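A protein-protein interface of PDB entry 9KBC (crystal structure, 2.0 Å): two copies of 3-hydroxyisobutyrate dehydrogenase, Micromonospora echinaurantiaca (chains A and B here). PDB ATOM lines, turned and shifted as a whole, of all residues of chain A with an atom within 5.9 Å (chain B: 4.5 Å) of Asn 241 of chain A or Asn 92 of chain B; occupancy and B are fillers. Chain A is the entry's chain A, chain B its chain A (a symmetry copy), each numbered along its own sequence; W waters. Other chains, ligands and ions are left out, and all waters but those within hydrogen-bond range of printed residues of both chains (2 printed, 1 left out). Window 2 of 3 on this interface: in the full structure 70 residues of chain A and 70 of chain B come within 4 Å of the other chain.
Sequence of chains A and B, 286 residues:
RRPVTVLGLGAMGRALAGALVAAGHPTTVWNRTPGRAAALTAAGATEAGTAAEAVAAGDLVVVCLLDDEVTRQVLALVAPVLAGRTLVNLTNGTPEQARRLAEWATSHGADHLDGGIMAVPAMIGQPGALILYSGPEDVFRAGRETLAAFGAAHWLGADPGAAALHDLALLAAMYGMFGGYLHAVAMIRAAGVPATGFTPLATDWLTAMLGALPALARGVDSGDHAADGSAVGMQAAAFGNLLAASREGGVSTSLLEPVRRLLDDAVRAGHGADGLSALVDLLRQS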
ATOM      1  N   ALA A 237      16.852 -17.052 -12.070  1.00  0.00           N
ATOM      2  CA  ALA A 237      17.656 -15.869 -11.782  1.00  0.00           C
ATOM      3  C   ALA A 237      16.788 -14.673 -11.412  1.00  0.00           C
ATOM      4  O   ALA A 237      17.238 -13.795 -10.667  1.00  0.00           O
ATOM      5  CB  ALA A 237      18.545 -15.531 -12.978  1.00  0.00           C
ATOM      6  N   ALA A 238      15.553 -14.619 -11.914  1.00  0.00           N
ATOM      7  CA  ALA A 238      14.638 -13.519 -11.627  1.00  0.00           C
ATOM      8  C   ALA A 238      13.815 -13.736 -10.362  1.00  0.00           C
ATOM      9  O   ALA A 238      13.177 -12.788  -9.885  1.00  0.00           O
ATOM     10  CB  ALA A 238      13.693 -13.298 -12.814  1.00  0.00           C
ATOM     11  N   PHE A 239      13.821 -14.952  -9.804  1.00  0.00           N
ATOM     12  CA  PHE A 239      13.017 -15.230  -8.619  1.00  0.00           C
ATOM     13  C   PHE A 239      13.538 -14.479  -7.402  1.00  0.00           C
ATOM     14  O   PHE A 239      12.756 -14.118  -6.515  1.00  0.00           O
ATOM     15  CB  PHE A 239      13.002 -16.736  -8.351  1.00  0.00           C
ATOM     16  CG  PHE A 239      11.713 -17.237  -7.780  1.00  0.00           C
ATOM     17  CD1 PHE A 239      11.362 -16.965  -6.469  1.00  0.00           C
ATOM     18  CD2 PHE A 239      10.854 -17.991  -8.553  1.00  0.00           C
ATOM     19  CE1 PHE A 239      10.174 -17.432  -5.945  1.00  0.00           C
ATOM     20  CE2 PHE A 239       9.664 -18.463  -8.034  1.00  0.00           C
ATOM     21  CZ  PHE A 239       9.323 -18.180  -6.729  1.00  0.00           C
ATOM     22  N   GLY A 240      14.848 -14.230  -7.349  1.00  0.00           N
ATOM     23  CA  GLY A 240      15.426 -13.582  -6.183  1.00  0.00           C
ATOM     24  C   GLY A 240      14.834 -12.212  -5.912  1.00  0.00           C
ATOM     25  O   GLY A 240      14.602 -11.846  -4.758  1.00  0.00           O
ATOM     26  N   ASN A 241      14.578 -11.439  -6.973  1.00  0.00           N
ATOM     27  CA  ASN A 241      13.995 -10.110  -6.791  1.00  0.00           C
ATOM     28  C   ASN A 241      12.580 -10.197  -6.238  1.00  0.00           C
ATOM     29  O   ASN A 241      12.158  -9.337  -5.457  1.00  0.00           O
ATOM     30  CB  ASN A 241      13.995  -9.341  -8.110  1.00  0.00           C
ATOM     31  CG  ASN A 241      15.365  -8.843  -8.492  1.00  0.00           C
ATOM     32  OD1 ASN A 241      16.012  -8.128  -7.725  1.00  0.00           O
ATOM     33  ND2 ASN A 241      15.816  -9.206  -9.687  1.00  0.00           N
ATOM     34  N   LEU A 242      11.826 -11.216  -6.653  1.00  0.00           N
ATOM     35  CA  LEU A 242      10.491 -11.425  -6.108  1.00  0.00           C
ATOM     36  C   LEU A 242      10.550 -11.685  -4.608  1.00  0.00           C
ATOM     37  O   LEU A 242       9.761 -11.130  -3.833  1.00  0.00           O
ATOM     38  CB  LEU A 242       9.815 -12.590  -6.834  1.00  0.00           C
ATOM     39  CG  LEU A 242       8.465 -13.085  -6.307  1.00  0.00           C
ATOM     40  CD1 LEU A 242       7.473 -11.940  -6.132  1.00  0.00           C
ATOM     41  CD2 LEU A 242       7.901 -14.163  -7.227  1.00  0.00           C
ATOM     42  N   LEU A 243      11.485 -12.538  -4.182  1.00  0.00           N
ATOM     43  CA  LEU A 243      11.642 -12.815  -2.759  1.00  0.00           C
ATOM     44  C   LEU A 243      12.090 -11.567  -2.007  1.00  0.00           C
ATOM     45  O   LEU A 243      11.592 -11.277  -0.913  1.00  0.00           O
ATOM     46  CB  LEU A 243      12.642 -13.954  -2.565  1.00  0.00           C
ATOM     47  CG  LEU A 243      12.264 -15.276  -3.232  1.00  0.00           C
ATOM     48  CD1 LEU A 243      13.419 -16.255  -3.139  1.00  0.00           C
ATOM     49  CD2 LEU A 243      11.006 -15.861  -2.609  1.00  0.00           C
ATOM     50  N   ALA A 244      13.031 -10.814  -2.583  1.00  0.00           N
ATOM     51  CA  ALA A 244      13.510  -9.599  -1.933  1.00  0.00           C
ATOM     52  C   ALA A 244      12.393  -8.569  -1.802  1.00  0.00           C
ATOM     53  O   ALA A 244      12.211  -7.962  -0.739  1.00  0.00           O
ATOM     54  CB  ALA A 244      14.692  -9.022  -2.710  1.00  0.00           C
ATOM     55  N   ALA A 245      11.627  -8.366  -2.877  1.00  0.00           N
ATOM     56  CA  ALA A 245      10.526  -7.409  -2.826  1.00  0.00           C
ATOM     57  C   ALA A 245       9.458  -7.840  -1.828  1.00  0.00           C
ATOM     58  O   ALA A 245       8.855  -7.000  -1.151  1.00  0.00           O
ATOM     59  CB  ALA A 245       9.921  -7.237  -4.215  1.00  0.00           C
ATOM     60  N   SER A 246       9.202  -9.147  -1.728  1.00  0.00           N
ATOM     61  CA  SER A 246       8.279  -9.634  -0.708  1.00  0.00           C
ATOM     62  C   SER A 246       8.787  -9.283   0.685  1.00  0.00           C
ATOM     63  O   SER A 246       8.027  -8.805   1.535  1.00  0.00           O
ATOM     64  CB  SER A 246       8.085 -11.145  -0.850  1.00  0.00           C
ATOM     65  OG  SER A 246       7.572 -11.476  -2.128  1.00  0.00           O
ATOM     66  N   ASP B  67      21.675  -6.379 -12.371  1.00  0.00           N
ATOM     67  CA  ASP B  67      20.869  -6.074 -11.198  1.00  0.00           C
ATOM     68  C   ASP B  67      21.135  -4.636 -10.765  1.00  0.00           C
ATOM     69  O   ASP B  67      21.910  -3.909 -11.391  1.00  0.00           O
ATOM     70  CB  ASP B  67      21.128  -7.087 -10.075  1.00  0.00           C
ATOM     71  CG  ASP B  67      22.555  -7.033  -9.539  1.00  0.00           C
ATOM     72  OD1 ASP B  67      23.333  -6.134  -9.925  1.00  0.00           O
ATOM     73  OD2 ASP B  67      22.898  -7.906  -8.715  1.00  0.00           O
ATOM     74  N   ASP B  68      20.483  -4.239  -9.672  1.00  0.00           N
ATOM     75  CA  ASP B  68      20.538  -2.848  -9.237  1.00  0.00           C
ATOM     76  C   ASP B  68      21.925  -2.447  -8.750  1.00  0.00           C
ATOM     77  O   ASP B  68      22.288  -1.269  -8.839  1.00  0.00           O
ATOM     78  CB  ASP B  68      19.491  -2.608  -8.150  1.00  0.00           C
ATOM     79  CG  ASP B  68      19.623  -1.248  -7.504  1.00  0.00           C
ATOM     80  OD1 ASP B  68      19.070  -0.272  -8.052  1.00  0.00           O
ATOM     81  OD2 ASP B  68      20.266  -1.160  -6.437  1.00  0.00           O
ATOM     82  N   LEU B  90      15.093  -0.413 -16.927  1.00  0.00           N
ATOM     83  CA  LEU B  90      14.456  -1.683 -17.237  1.00  0.00           C
ATOM     84  C   LEU B  90      15.129  -2.848 -16.521  1.00  0.00           C
ATOM     85  O   LEU B  90      14.764  -4.003 -16.756  1.00  0.00           O
ATOM     86  CB  LEU B  90      14.459  -1.914 -18.747  1.00  0.00           C
ATOM     87  CG  LEU B  90      13.649  -0.894 -19.553  1.00  0.00           C
ATOM     88  CD1 LEU B  90      13.503  -1.330 -21.002  1.00  0.00           C
ATOM     89  CD2 LEU B  90      12.293  -0.657 -18.920  1.00  0.00           C
ATOM     90  N   THR B  91      16.101  -2.562 -15.656  1.00  0.00           N
ATOM     91  CA  THR B  91      16.801  -3.597 -14.907  1.00  0.00           C
ATOM     92  C   THR B  91      15.883  -4.211 -13.860  1.00  0.00           C
ATOM     93  O   THR B  91      15.214  -3.494 -13.108  1.00  0.00           O
ATOM     94  CB  THR B  91      18.038  -3.011 -14.225  1.00  0.00           C
ATOM     95  OG1 THR B  91      18.956  -2.521 -15.214  1.00  0.00           O
ATOM     96  CG2 THR B  91      18.725  -4.061 -13.361  1.00  0.00           C
ATOM     97  N   ASN B  92      15.867  -5.539 -13.799  1.00  0.00           N
ATOM     98  CA  ASN B  92      15.063  -6.227 -12.800  1.00  0.00           C
ATOM     99  C   ASN B  92      15.548  -5.873 -11.405  1.00  0.00           C
ATOM    100  O   ASN B  92      16.739  -5.990 -11.101  1.00  0.00           O
ATOM    101  CB  ASN B  92      15.123  -7.740 -13.013  1.00  0.00           C
ATOM    102  CG  ASN B  92      14.272  -8.192 -14.179  1.00  0.00           C
ATOM    103  OD1 ASN B  92      13.454  -7.428 -14.693  1.00  0.00           O
ATOM    104  ND2 ASN B  92      14.458  -9.439 -14.607  1.00  0.00           N
ATOM    105  N   GLY B  93      14.620  -5.439 -10.562  1.00  0.00           N
ATOM    106  CA  GLY B  93      14.960  -5.033  -9.221  1.00  0.00           C
ATOM    107  C   GLY B  93      13.726  -4.933  -8.357  1.00  0.00           C
ATOM    108  O   GLY B  93      12.649  -5.407  -8.724  1.00  0.00           O
ATOM    109  N   THR B  94      13.897  -4.299  -7.205  1.00  0.00           N
ATOM    110  CA  THR B  94      12.831  -4.158  -6.231  1.00  0.00           C
ATOM    111  C   THR B  94      12.215  -2.766  -6.294  1.00  0.00           C
ATOM    112  O   THR B  94      12.822  -1.828  -6.821  1.00  0.00           O
ATOM    113  CB  THR B  94      13.367  -4.424  -4.823  1.00  0.00           C
ATOM    114  OG1 THR B  94      14.118  -3.296  -4.374  1.00  0.00           O
ATOM    115  CG2 THR B  94      14.272  -5.655  -4.820  1.00  0.00           C
ATOM    116  N   GLN B  97      14.531  -0.318  -4.543  1.00  0.00           N
ATOM    117  CA  GLN B  97      15.674  -0.001  -5.392  1.00  0.00           C
ATOM    118  C   GLN B  97      15.292   1.028  -6.451  1.00  0.00           C
ATOM    119  O   GLN B  97      16.039   1.980  -6.712  1.00  0.00           O
ATOM    120  CB  GLN B  97      16.209  -1.276  -6.042  1.00  0.00           C
ATOM    121  CG  GLN B  97      17.012  -2.152  -5.098  1.00  0.00           C
ATOM    122  CD  GLN B  97      17.240  -3.549  -5.643  1.00  0.00           C
ATOM    123  OE1 GLN B  97      16.742  -3.905  -6.715  1.00  0.00           O
ATOM    124  NE2 GLN B  97      18.005  -4.347  -4.911  1.00  0.00           N
ATOM    125  N   LEU B 168       6.562  -7.936 -10.299  1.00  0.00           N
ATOM    126  CA  LEU B 168       6.855  -9.067  -9.429  1.00  0.00           C
ATOM    127  C   LEU B 168       5.585  -9.675  -8.847  1.00  0.00           C
ATOM    128  O   LEU B 168       5.528 -10.891  -8.637  1.00  0.00           O
ATOM    129  CB  LEU B 168       7.808  -8.631  -8.318  1.00  0.00           C
ATOM    130  CG  LEU B 168       9.128  -8.062  -8.849  1.00  0.00           C
ATOM    131  CD1 LEU B 168       9.966  -7.513  -7.719  1.00  0.00           C
ATOM    132  CD2 LEU B 168       9.901  -9.113  -9.636  1.00  0.00           C
HETATM  133  O   HOH W   1      17.305  -7.568  -5.233  1.00  0.00           O
HETATM  134  O   HOH W   2      18.257  -8.768 -11.000  1.00  0.00           O
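Among the printed residues, merely in contact across the chains: Asn 241 of chain A with Asn 92 of chain B, Asn 241 of chain A with Gly 93 of chain B, Asn 241 of chain A with Leu 168 of chain B, Leu 242 of chain A with Leu 168 of chain B, Ala 244 of chain A with Thr 94 of chain B and Ala 245 of chain A with Leu 168 of chain B.
O of Leu 242 of chain A sits at hydrogen-bond distance from OG of Ser 246 of chain A (2.8 Å). The backbone NH (N) of Thr 94 of chain B lies within hydrogen-bond range of the side-chain amide oxygen (OE1) of Gln 97 of chain B.
Gly 240 of chain A touches none of the printed residues of chain B. Asn 241 of chain A touches just these residues of chain B: Asn 92, Gly 93 and Leu 168. Printed residues of chain B within 4 Å of Leu 242 of chain A: Leu 168. Of the printed residues of chain B, Ala 244 of chain A touches Thr 94 (3.996 Å). Of the printed residues of chain B, Ala 245 of chain A touches Leu 168 (3.5 Å). Printed residues of chain A within 4 Å of Leu 168 of chain B: Asn 241 (3.6 Å), Leu 242 (3.3 Å) and Ala 245 (3.5 Å). The nearest residue of chain B that does not touch Asn 241 of chain A is Thr 94 of chain B (4.2 Å). The nearest residue of chain A that does not touch Asn 92 of chain B is Ala 238 of chain A (4.3 Å).
No position is printed for both chains. Of the 6 pairs that touch across the chains among the printed residues, none has its exchanged pair printed and touching as well.
Water W2 lies within hydrogen-bond range of ND2 of Asn 241 of chain A (2.8 Å) and O of Asn 92 of chain B (3.2 Å). Water W1 lies within hydrogen-bond range of OD1 of Asn 241 of chain A and NE2 of Gln 97 of chain B.
Hydrophobic or aromatic side chains of chain A within 4 Å of the printed part of chain B: Leu 242, Ala 244 and Ala 245. Printed residues of chain B that touch a printed residue of chain A: Asn 92, Gly 93, Thr 94 and Leu 168. Among the printed residues, no Asp or Glu carboxylate lies within 4 Å of a Lys or Arg side-chain nitrogen of the other chain.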
